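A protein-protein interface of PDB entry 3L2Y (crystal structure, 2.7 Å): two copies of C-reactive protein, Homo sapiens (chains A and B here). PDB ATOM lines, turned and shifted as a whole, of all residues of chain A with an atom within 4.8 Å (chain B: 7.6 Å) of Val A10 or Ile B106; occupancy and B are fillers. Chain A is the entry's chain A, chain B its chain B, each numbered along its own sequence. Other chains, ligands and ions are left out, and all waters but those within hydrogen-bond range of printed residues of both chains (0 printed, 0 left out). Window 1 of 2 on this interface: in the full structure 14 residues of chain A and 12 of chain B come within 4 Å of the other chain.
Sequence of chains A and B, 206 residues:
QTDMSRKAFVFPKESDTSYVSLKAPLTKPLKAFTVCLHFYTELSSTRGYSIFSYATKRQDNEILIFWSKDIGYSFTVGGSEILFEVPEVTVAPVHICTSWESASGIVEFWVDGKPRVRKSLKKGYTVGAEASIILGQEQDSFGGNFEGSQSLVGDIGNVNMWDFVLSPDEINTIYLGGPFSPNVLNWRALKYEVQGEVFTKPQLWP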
ATOM      1  N   ALA A   8     -18.992 -20.014 -13.179  1.00  0.00           N
ATOM      2  CA  ALA A   8     -19.841 -19.879 -14.356  1.00  0.00           C
ATOM      3  C   ALA A   8     -19.027 -20.020 -15.616  1.00  0.00           C
ATOM      4  O   ALA A   8     -17.824 -19.778 -15.606  1.00  0.00           O
ATOM      5  CB  ALA A   8     -20.536 -18.546 -14.343  1.00  0.00           C
ATOM      6  N   PHE A   9     -19.681 -20.408 -16.707  1.00  0.00           N
ATOM      7  CA  PHE A   9     -19.013 -20.447 -17.998  1.00  0.00           C
ATOM      8  C   PHE A   9     -19.118 -19.070 -18.621  1.00  0.00           C
ATOM      9  O   PHE A   9     -20.163 -18.427 -18.515  1.00  0.00           O
ATOM     10  CB  PHE A   9     -19.633 -21.505 -18.908  1.00  0.00           C
ATOM     11  CG  PHE A   9     -19.356 -22.918 -18.477  1.00  0.00           C
ATOM     12  CD1 PHE A   9     -18.061 -23.382 -18.362  1.00  0.00           C
ATOM     13  CD2 PHE A   9     -20.395 -23.787 -18.203  1.00  0.00           C
ATOM     14  CE1 PHE A   9     -17.805 -24.691 -17.968  1.00  0.00           C
ATOM     15  CE2 PHE A   9     -20.145 -25.101 -17.809  1.00  0.00           C
ATOM     16  CZ  PHE A   9     -18.848 -25.549 -17.697  1.00  0.00           C
ATOM     17  N   VAL A  10     -18.041 -18.617 -19.258  1.00  0.00           N
ATOM     18  CA  VAL A  10     -18.020 -17.306 -19.871  1.00  0.00           C
ATOM     19  C   VAL A  10     -17.767 -17.430 -21.351  1.00  0.00           C
ATOM     20  O   VAL A  10     -16.803 -18.056 -21.762  1.00  0.00           O
ATOM     21  CB  VAL A  10     -16.919 -16.415 -19.256  1.00  0.00           C
ATOM     22  CG1 VAL A  10     -16.978 -15.017 -19.835  1.00  0.00           C
ATOM     23  CG2 VAL A  10     -17.053 -16.353 -17.738  1.00  0.00           C
ATOM     24  N   PHE A  11     -18.647 -16.827 -22.150  1.00  0.00           N
ATOM     25  CA  PHE A  11     -18.499 -16.762 -23.607  1.00  0.00           C
ATOM     26  C   PHE A  11     -18.333 -15.304 -23.975  1.00  0.00           C
ATOM     27  O   PHE A  11     -19.314 -14.627 -24.277  1.00  0.00           O
ATOM     28  CB  PHE A  11     -19.736 -17.343 -24.315  1.00  0.00           C
ATOM     29  CG  PHE A  11     -20.098 -18.729 -23.862  1.00  0.00           C
ATOM     30  CD1 PHE A  11     -19.704 -19.836 -24.588  1.00  0.00           C
ATOM     31  CD2 PHE A  11     -20.805 -18.927 -22.690  1.00  0.00           C
ATOM     32  CE1 PHE A  11     -20.026 -21.118 -24.164  1.00  0.00           C
ATOM     33  CE2 PHE A  11     -21.127 -20.206 -22.254  1.00  0.00           C
ATOM     34  CZ  PHE A  11     -20.741 -21.301 -22.996  1.00  0.00           C
ATOM     35  N   PRO A  12     -17.085 -14.818 -23.951  1.00  0.00           N
ATOM     36  CA  PRO A  12     -16.717 -13.404 -24.067  1.00  0.00           C
ATOM     37  C   PRO A  12     -17.097 -12.714 -25.398  1.00  0.00           C
ATOM     38  O   PRO A  12     -17.389 -11.513 -25.384  1.00  0.00           O
ATOM     39  CB  PRO A  12     -15.197 -13.432 -23.901  1.00  0.00           C
ATOM     40  CG  PRO A  12     -14.898 -14.746 -23.277  1.00  0.00           C
ATOM     41  CD  PRO A  12     -15.899 -15.673 -23.823  1.00  0.00           C
ATOM     42  N   GLY A 154     -21.881 -13.881 -23.008  1.00  0.00           N
ATOM     43  CA  GLY A 154     -22.034 -13.544 -21.610  1.00  0.00           C
ATOM     44  C   GLY A 154     -21.743 -14.734 -20.726  1.00  0.00           C
ATOM     45  O   GLY A 154     -20.894 -15.566 -21.060  1.00  0.00           O
ATOM     46  N   ASP A 155     -22.444 -14.815 -19.598  1.00  0.00           N
ATOM     47  CA  ASP A 155     -22.196 -15.871 -18.621  1.00  0.00           C
ATOM     48  C   ASP A 155     -23.400 -16.793 -18.491  1.00  0.00           C
ATOM     49  O   ASP A 155     -24.549 -16.371 -18.642  1.00  0.00           O
ATOM     50  CB  ASP A 155     -21.884 -15.296 -17.231  1.00  0.00           C
ATOM     51  CG  ASP A 155     -20.605 -14.479 -17.189  1.00  0.00           C
ATOM     52  OD1 ASP A 155     -20.288 -13.774 -18.172  1.00  0.00           O
ATOM     53  OD2 ASP A 155     -19.933 -14.526 -16.141  1.00  0.00           O
ATOM     54  N   GLU A 197     -13.661 -20.990 -27.439  1.00  0.00           N
ATOM     55  CA  GLU A 197     -13.371 -19.854 -26.573  1.00  0.00           C
ATOM     56  C   GLU A 197     -14.348 -19.755 -25.392  1.00  0.00           C
ATOM     57  O   GLU A 197     -15.204 -18.876 -25.365  1.00  0.00           O
ATOM     58  CB  GLU A 197     -13.423 -18.573 -27.411  1.00  0.00           C
ATOM     59  CG  GLU A 197     -12.613 -17.403 -26.886  1.00  0.00           C
ATOM     60  CD  GLU A 197     -11.117 -17.581 -27.110  1.00  0.00           C
ATOM     61  OE1 GLU A 197     -10.667 -18.742 -27.294  1.00  0.00           O
ATOM     62  OE2 GLU A 197     -10.398 -16.553 -27.104  1.00  0.00           O
ATOM     63  N   VAL A 198     -14.207 -20.660 -24.425  1.00  0.00           N
ATOM     64  CA  VAL A 198     -15.034 -20.691 -23.217  1.00  0.00           C
ATOM     65  C   VAL A 198     -14.162 -20.682 -21.961  1.00  0.00           C
ATOM     66  O   VAL A 198     -13.173 -21.417 -21.869  1.00  0.00           O
ATOM     67  CB  VAL A 198     -15.886 -21.963 -23.165  1.00  0.00           C
ATOM     68  CG1 VAL A 198     -16.770 -21.955 -21.932  1.00  0.00           C
ATOM     69  CG2 VAL A 198     -16.717 -22.101 -24.426  1.00  0.00           C
ATOM     70  N   PHE A 199     -14.528 -19.866 -20.983  1.00  0.00           N
ATOM     71  CA  PHE A 199     -13.728 -19.775 -19.775  1.00  0.00           C
ATOM     72  C   PHE A 199     -14.547 -20.049 -18.539  1.00  0.00           C
ATOM     73  O   PHE A 199     -15.769 -19.856 -18.530  1.00  0.00           O
ATOM     74  CB  PHE A 199     -13.068 -18.399 -19.669  1.00  0.00           C
ATOM     75  CG  PHE A 199     -12.268 -18.035 -20.870  1.00  0.00           C
ATOM     76  CD1 PHE A 199     -10.960 -18.466 -21.002  1.00  0.00           C
ATOM     77  CD2 PHE A 199     -12.826 -17.291 -21.886  1.00  0.00           C
ATOM     78  CE1 PHE A 199     -10.221 -18.147 -22.131  1.00  0.00           C
ATOM     79  CE2 PHE A 199     -12.103 -16.971 -23.005  1.00  0.00           C
ATOM     80  CZ  PHE A 199     -10.799 -17.399 -23.130  1.00  0.00           C
ATOM     81  N   LYS A 201     -14.998 -18.850 -14.773  1.00  0.00           N
ATOM     82  CA  LYS A 201     -14.726 -17.744 -13.869  1.00  0.00           C
ATOM     83  C   LYS A 201     -15.703 -17.750 -12.704  1.00  0.00           C
ATOM     84  O   LYS A 201     -16.718 -18.418 -12.754  1.00  0.00           O
ATOM     85  CB  LYS A 201     -14.836 -16.425 -14.625  1.00  0.00           C
ATOM     86  CG  LYS A 201     -13.791 -16.244 -15.722  1.00  0.00           C
ATOM     87  CD  LYS A 201     -12.398 -16.225 -15.141  1.00  0.00           C
ATOM     88  CE  LYS A 201     -11.373 -15.762 -16.150  1.00  0.00           C
ATOM     89  NZ  LYS A 201     -10.012 -15.693 -15.532  1.00  0.00           N
ATOM     90  N   PHE B  33      -5.116  -6.425 -14.979  1.00  0.00           N
ATOM     91  CA  PHE B  33      -5.224  -5.281 -14.074  1.00  0.00           C
ATOM     92  C   PHE B  33      -6.652  -5.005 -13.639  1.00  0.00           C
ATOM     93  O   PHE B  33      -7.605  -5.445 -14.283  1.00  0.00           O
ATOM     94  CB  PHE B  33      -4.627  -4.011 -14.703  1.00  0.00           C
ATOM     95  CG  PHE B  33      -5.419  -3.465 -15.855  1.00  0.00           C
ATOM     96  CD1 PHE B  33      -6.536  -2.668 -15.634  1.00  0.00           C
ATOM     97  CD2 PHE B  33      -5.044  -3.726 -17.161  1.00  0.00           C
ATOM     98  CE1 PHE B  33      -7.264  -2.158 -16.692  1.00  0.00           C
ATOM     99  CE2 PHE B  33      -5.777  -3.222 -18.217  1.00  0.00           C
ATOM    100  CZ  PHE B  33      -6.889  -2.437 -17.977  1.00  0.00           C
ATOM    101  N   PHE B  75     -14.382   1.638 -22.795  1.00  0.00           N
ATOM    102  CA  PHE B  75     -13.202   1.061 -22.171  1.00  0.00           C
ATOM    103  C   PHE B  75     -12.200   0.657 -23.252  1.00  0.00           C
ATOM    104  O   PHE B  75     -12.532  -0.092 -24.165  1.00  0.00           O
ATOM    105  CB  PHE B  75     -13.608  -0.141 -21.322  1.00  0.00           C
ATOM    106  CG  PHE B  75     -12.480  -0.779 -20.575  1.00  0.00           C
ATOM    107  CD1 PHE B  75     -11.815  -0.084 -19.589  1.00  0.00           C
ATOM    108  CD2 PHE B  75     -12.106  -2.102 -20.832  1.00  0.00           C
ATOM    109  CE1 PHE B  75     -10.779  -0.679 -18.873  1.00  0.00           C
ATOM    110  CE2 PHE B  75     -11.070  -2.705 -20.129  1.00  0.00           C
ATOM    111  CZ  PHE B  75     -10.398  -1.996 -19.149  1.00  0.00           C
ATOM    112  N   ILE B  82     -14.142  -1.059 -26.500  1.00  0.00           N
ATOM    113  CA  ILE B  82     -15.495  -1.613 -26.418  1.00  0.00           C
ATOM    114  C   ILE B  82     -16.374  -0.665 -25.634  1.00  0.00           C
ATOM    115  O   ILE B  82     -15.879   0.168 -24.897  1.00  0.00           O
ATOM    116  CB  ILE B  82     -15.568  -2.952 -25.702  1.00  0.00           C
ATOM    117  CG1 ILE B  82     -14.837  -2.863 -24.380  1.00  0.00           C
ATOM    118  CG2 ILE B  82     -15.014  -4.050 -26.560  1.00  0.00           C
ATOM    119  CD1 ILE B  82     -14.960  -4.104 -23.608  1.00  0.00           C
ATOM    120  N   SER B  99     -11.762  -4.184 -15.100  1.00  0.00           N
ATOM    121  CA  SER B  99     -10.654  -5.146 -15.126  1.00  0.00           C
ATOM    122  C   SER B  99     -10.472  -5.793 -16.481  1.00  0.00           C
ATOM    123  O   SER B  99     -11.388  -5.837 -17.298  1.00  0.00           O
ATOM    124  CB  SER B  99     -10.833  -6.232 -14.067  1.00  0.00           C
ATOM    125  OG  SER B  99     -11.835  -7.175 -14.436  1.00  0.00           O
ATOM    126  N   TRP B 100      -9.269  -6.286 -16.711  1.00  0.00           N
ATOM    127  CA  TRP B 100      -8.930  -6.937 -17.963  1.00  0.00           C
ATOM    128  C   TRP B 100      -7.883  -8.007 -17.726  1.00  0.00           C
ATOM    129  O   TRP B 100      -6.954  -7.803 -16.952  1.00  0.00           O
ATOM    130  CB  TRP B 100      -8.373  -5.919 -18.930  1.00  0.00           C
ATOM    131  CG  TRP B 100      -7.642  -6.518 -20.107  1.00  0.00           C
ATOM    132  CD1 TRP B 100      -8.183  -6.926 -21.288  1.00  0.00           C
ATOM    133  CD2 TRP B 100      -6.235  -6.727 -20.221  1.00  0.00           C
ATOM    134  NE1 TRP B 100      -7.203  -7.380 -22.130  1.00  0.00           N
ATOM    135  CE2 TRP B 100      -5.994  -7.267 -21.499  1.00  0.00           C
ATOM    136  CE3 TRP B 100      -5.152  -6.510 -19.368  1.00  0.00           C
ATOM    137  CZ2 TRP B 100      -4.719  -7.605 -21.936  1.00  0.00           C
ATOM    138  CZ3 TRP B 100      -3.895  -6.832 -19.809  1.00  0.00           C
ATOM    139  CH2 TRP B 100      -3.689  -7.375 -21.081  1.00  0.00           C
ATOM    140  N   GLU B 101      -8.038  -9.147 -18.391  1.00  0.00           N
ATOM    141  CA  GLU B 101      -7.091 -10.252 -18.272  1.00  0.00           C
ATOM    142  C   GLU B 101      -6.575 -10.650 -19.650  1.00  0.00           C
ATOM    143  O   GLU B 101      -7.351 -10.941 -20.550  1.00  0.00           O
ATOM    144  CB  GLU B 101      -7.753 -11.448 -17.597  1.00  0.00           C
ATOM    145  CG  GLU B 101      -6.811 -12.609 -17.347  1.00  0.00           C
ATOM    146  CD  GLU B 101      -7.527 -13.855 -16.874  1.00  0.00           C
ATOM    147  OE1 GLU B 101      -8.639 -14.133 -17.379  1.00  0.00           O
ATOM    148  OE2 GLU B 101      -6.976 -14.551 -15.993  1.00  0.00           O
ATOM    149  N   SER B 102      -5.264 -10.653 -19.824  1.00  0.00           N
ATOM    150  CA  SER B 102      -4.684 -11.007 -21.111  1.00  0.00           C
ATOM    151  C   SER B 102      -4.982 -12.453 -21.491  1.00  0.00           C
ATOM    152  O   SER B 102      -5.340 -12.749 -22.632  1.00  0.00           O
ATOM    153  CB  SER B 102      -3.172 -10.809 -21.095  1.00  0.00           C
ATOM    154  OG  SER B 102      -2.619 -11.217 -22.332  1.00  0.00           O
ATOM    155  N   ALA B 103      -4.813 -13.351 -20.527  1.00  0.00           N
ATOM    156  CA  ALA B 103      -5.043 -14.772 -20.769  1.00  0.00           C
ATOM    157  C   ALA B 103      -6.367 -15.087 -21.493  1.00  0.00           C
ATOM    158  O   ALA B 103      -6.401 -15.972 -22.359  1.00  0.00           O
ATOM    159  CB  ALA B 103      -4.956 -15.544 -19.461  1.00  0.00           C
ATOM    160  N   SER B 104      -7.444 -14.376 -21.136  1.00  0.00           N
ATOM    161  CA  SER B 104      -8.780 -14.684 -21.645  1.00  0.00           C
ATOM    162  C   SER B 104      -9.361 -13.579 -22.512  1.00  0.00           C
ATOM    163  O   SER B 104     -10.243 -13.823 -23.344  1.00  0.00           O
ATOM    164  CB  SER B 104      -9.732 -14.953 -20.489  1.00  0.00           C
ATOM    165  OG  SER B 104      -9.905 -13.787 -19.713  1.00  0.00           O
ATOM    166  N   GLY B 105      -8.884 -12.358 -22.308  1.00  0.00           N
ATOM    167  CA  GLY B 105      -9.400 -11.213 -23.032  1.00  0.00           C
ATOM    168  C   GLY B 105     -10.645 -10.668 -22.360  1.00  0.00           C
ATOM    169  O   GLY B 105     -11.279  -9.740 -22.856  1.00  0.00           O
ATOM    170  N   ILE B 106     -10.994 -11.241 -21.220  1.00  0.00           N
ATOM    171  CA  ILE B 106     -12.220 -10.863 -20.539  1.00  0.00           C
ATOM    172  C   ILE B 106     -12.084  -9.518 -19.855  1.00  0.00           C
ATOM    173  O   ILE B 106     -11.167  -9.325 -19.065  1.00  0.00           O
ATOM    174  CB  ILE B 106     -12.613 -11.925 -19.490  1.00  0.00           C
ATOM    175  CG1 ILE B 106     -13.116 -13.184 -20.191  1.00  0.00           C
ATOM    176  CG2 ILE B 106     -13.684 -11.407 -18.570  1.00  0.00           C
ATOM    177  CD1 ILE B 106     -13.467 -14.279 -19.226  1.00  0.00           C
ATOM    178  N   VAL B 107     -12.990  -8.583 -20.144  1.00  0.00           N
ATOM    179  CA  VAL B 107     -13.040  -7.358 -19.358  1.00  0.00           C
ATOM    180  C   VAL B 107     -14.306  -7.327 -18.520  1.00  0.00           C
ATOM    181  O   VAL B 107     -15.338  -7.854 -18.928  1.00  0.00           O
ATOM    182  CB  VAL B 107     -12.914  -6.081 -20.205  1.00  0.00           C
ATOM    183  CG1 VAL B 107     -11.908  -6.274 -21.320  1.00  0.00           C
ATOM    184  CG2 VAL B 107     -14.240  -5.685 -20.761  1.00  0.00           C
ATOM    185  N   GLU B 108     -14.211  -6.747 -17.329  1.00  0.00           N
ATOM    186  CA  GLU B 108     -15.366  -6.588 -16.472  1.00  0.00           C
ATOM    187  C   GLU B 108     -15.577  -5.110 -16.251  1.00  0.00           C
ATOM    188  O   GLU B 108     -14.617  -4.358 -16.158  1.00  0.00           O
ATOM    189  CB  GLU B 108     -15.148  -7.292 -15.133  1.00  0.00           C
ATOM    190  CG  GLU B 108     -15.184  -8.799 -15.225  1.00  0.00           C
ATOM    191  CD  GLU B 108     -14.996  -9.473 -13.897  1.00  0.00           C
ATOM    192  OE1 GLU B 108     -14.972  -8.771 -12.858  1.00  0.00           O
ATOM    193  OE2 GLU B 108     -14.857 -10.715 -13.901  1.00  0.00           O
ATOM    194  N   VAL B 117     -22.280  -7.000 -17.964  1.00  0.00           N
ATOM    195  CA  VAL B 117     -21.926  -8.273 -18.551  1.00  0.00           C
ATOM    196  C   VAL B 117     -20.431  -8.329 -18.894  1.00  0.00           C
ATOM    197  O   VAL B 117     -19.780  -7.318 -19.033  1.00  0.00           O
ATOM    198  CB  VAL B 117     -22.777  -8.574 -19.800  1.00  0.00           C
ATOM    199  CG1 VAL B 117     -22.233  -7.842 -20.994  1.00  0.00           C
ATOM    200  CG2 VAL B 117     -22.772 -10.058 -20.079  1.00  0.00           C
ATOM    201  N   ARG B 118     -19.878  -9.525 -18.998  1.00  0.00           N
ATOM    202  CA  ARG B 118     -18.490  -9.657 -19.365  1.00  0.00           C
ATOM    203  C   ARG B 118     -18.303  -9.544 -20.876  1.00  0.00           C
ATOM    204  O   ARG B 118     -19.154  -9.977 -21.665  1.00  0.00           O
ATOM    205  CB  ARG B 118     -17.950 -10.977 -18.863  1.00  0.00           C
ATOM    206  CG  ARG B 118     -17.692 -10.995 -17.372  1.00  0.00           C
ATOM    207  CD  ARG B 118     -17.353 -12.399 -16.858  1.00  0.00           C
ATOM    208  NE  ARG B 118     -16.742 -12.371 -15.528  1.00  0.00           N
ATOM    209  CZ  ARG B 118     -17.090 -13.158 -14.513  1.00  0.00           C
ATOM    210  NH1 ARG B 118     -18.061 -14.051 -14.656  1.00  0.00           N
ATOM    211  NH2 ARG B 118     -16.462 -13.053 -13.349  1.00  0.00           N
ATOM    212  N   LYS B 119     -17.192  -8.945 -21.284  1.00  0.00           N
ATOM    213  CA  LYS B 119     -16.911  -8.778 -22.705  1.00  0.00           C
ATOM    214  C   LYS B 119     -15.464  -9.148 -23.030  1.00  0.00           C
ATOM    215  O   LYS B 119     -14.684  -9.470 -22.140  1.00  0.00           O
ATOM    216  CB  LYS B 119     -17.216  -7.343 -23.161  1.00  0.00           C
ATOM    217  CG  LYS B 119     -18.639  -6.886 -22.848  1.00  0.00           C
ATOM    218  CD  LYS B 119     -19.029  -5.629 -23.629  1.00  0.00           C
ATOM    219  CE  LYS B 119     -20.507  -5.302 -23.446  1.00  0.00           C
ATOM    220  NZ  LYS B 119     -21.051  -4.340 -24.448  1.00  0.00           N
ATOM    221  N   SER B 120     -15.112  -9.083 -24.307  1.00  0.00           N
ATOM    222  CA  SER B 120     -13.799  -9.509 -24.753  1.00  0.00           C
ATOM    223  C   SER B 120     -13.007  -8.352 -25.339  1.00  0.00           C
ATOM    224  O   SER B 120     -13.540  -7.538 -26.088  1.00  0.00           O
ATOM    225  CB  SER B 120     -13.930 -10.617 -25.802  1.00  0.00           C
ATOM    226  OG  SER B 120     -12.684 -11.257 -26.020  1.00  0.00           O
ATOM    227  N   LEU B 121     -11.723  -8.297 -25.015  1.00  0.00           N
ATOM    228  CA  LEU B 121     -10.870  -7.235 -25.509  1.00  0.00           C
ATOM    229  C   LEU B 121      -9.393  -7.616 -25.421  1.00  0.00           C
ATOM    230  O   LEU B 121      -8.894  -7.978 -24.353  1.00  0.00           O
ATOM    231  CB  LEU B 121     -11.122  -5.980 -24.691  1.00  0.00           C
ATOM    232  CG  LEU B 121     -10.569  -4.700 -25.272  1.00  0.00           C
ATOM    233  CD1 LEU B 121     -11.155  -4.489 -26.654  1.00  0.00           C
ATOM    234  CD2 LEU B 121     -10.944  -3.581 -24.337  1.00  0.00           C
ATOM    235  N   LYS B 122      -8.705  -7.546 -26.556  1.00  0.00           N
ATOM    236  CA  LYS B 122      -7.259  -7.731 -26.595  1.00  0.00           C
ATOM    237  C   LYS B 122      -6.729  -8.991 -25.887  1.00  0.00           C
ATOM    238  O   LYS B 122      -5.829  -8.897 -25.040  1.00  0.00           O
ATOM    239  CB  LYS B 122      -6.570  -6.488 -26.010  1.00  0.00           C
ATOM    240  CG  LYS B 122      -6.479  -5.296 -26.965  1.00  0.00           C
ATOM    241  CD  LYS B 122      -5.354  -5.498 -27.982  1.00  0.00           C
ATOM    242  CE  LYS B 122      -5.269  -4.356 -28.971  1.00  0.00           C
ATOM    243  NZ  LYS B 122      -4.024  -4.421 -29.767  1.00  0.00           N
ATOM    244  N   LYS B 123      -7.257 -10.164 -26.236  1.00  0.00           N
ATOM    245  CA  LYS B 123      -6.722 -11.412 -25.694  1.00  0.00           C
ATOM    246  C   LYS B 123      -5.254 -11.555 -26.082  1.00  0.00           C
ATOM    247  O   LYS B 123      -4.900 -11.379 -27.248  1.00  0.00           O
ATOM    248  CB  LYS B 123      -7.505 -12.616 -26.208  1.00  0.00           C
ATOM    249  CG  LYS B 123      -7.083 -13.929 -25.561  1.00  0.00           C
ATOM    250  CD  LYS B 123      -7.826 -15.131 -26.148  1.00  0.00           C
ATOM    251  CE  LYS B 123      -7.365 -16.428 -25.478  1.00  0.00           C
ATOM    252  NZ  LYS B 123      -7.961 -17.655 -26.087  1.00  0.00           N
ATOM    253  N   VAL B 165      -6.774  -9.407 -11.634  1.00  0.00           N
ATOM    254  CA  VAL B 165      -8.214  -9.209 -11.665  1.00  0.00           C
ATOM    255  C   VAL B 165      -8.859  -9.460 -10.306  1.00  0.00           C
ATOM    256  O   VAL B 165      -8.729 -10.542  -9.724  1.00  0.00           O
ATOM    257  CB  VAL B 165      -8.898 -10.098 -12.716  1.00  0.00           C
ATOM    258  CG1 VAL B 165     -10.374  -9.885 -12.688  1.00  0.00           C
ATOM    259  CG2 VAL B 165      -8.367  -9.801 -14.089  1.00  0.00           C
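The backbone NH of Phe A11 lies within hydrogen-bond range of the backbone carbonyl oxygen of Gly A154 (2.8 Å).
The side-chain hydroxyl (OG) of Ser B104 lies within hydrogen-bond range of the side-chain carboxylate (OE1) of Glu B101.
The backbone NH (N) of Val A10 sits at hydrogen-bond distance from the backbone carbonyl oxygen (O) of Phe A199, 2.7 Å away.
N of Ala A8 sits at hydrogen-bond distance from O of Lys A201, at 2.8 Å.
The backbone NH (N) of Glu B101 is in hydrogen-bond range of the backbone carbonyl oxygen (O) of Ile B106.
The backbone NH of Ile B106 sits close to the side-chain hydroxyl of Ser B104.
Among the printed residues, pairs that only touch across the chains: Val A10 with Ile B106, Val A10 with Arg B118, Pro A12 with Ile B106, Pro A12 with Lys B119, Gly A154 with Val B117, Phe A199 with Ser B104 and Lys A201 with Arg B118.
Hydrophobic or aromatic side chains of chain B within 4 Å of the printed part of chain A: Ile B106 and Val B117.
Hydrophobic or aromatic side chains of chain A that line the printed part of chain B: Val A10, Pro A12 and Phe A199.
Among the printed residues, 11 pairs touch across the chains.
No position is printed for both chains.
OE2 of Glu A197 lies within salt-bridge range of NZ of Lys B123, 2.9 Å away.
NH1 of Arg B118 is in salt-bridge range of OD2 of Asp A155, 2.4 Å away.
The side-chain amino group of Lys A201 is in salt-bridge range of the side-chain carboxylate of Glu B101 (2.8 Å).
N of Ser B120 lies within hydrogen-bond range of O of Pro A12 (3.5 Å).
Val A10 touches two residues of chain B.
Of the printed residues of chain A, Ile B106 touches Val A10 (3.6 Å) and Pro A12 (3.9 Å).
Printed residues of chain A within 4 Å of Ser B120: Pro A12 (3.5 Å).
Printed residues of chain A within 4 Å of Lys B123: Glu A197.
Printed residues of chain A within 4 Å of Ser B104: Phe A199 (3.6 Å).
Printed residues of chain B within 4 Å of Lys A201: Glu B101 (2.8 Å) and Arg B118 (3.96 Å).
Of the printed residues of chain B, Asp A155 touches Arg B118.
Leu B121 touches none of the printed residues of chain A.
The nearest printed residue of chain A that does not touch Ile B106 is Lys A201 (4.01 Å).
The nearest printed residue of chain B that does not touch Pro A12 is Arg B118 (4.4 Å).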
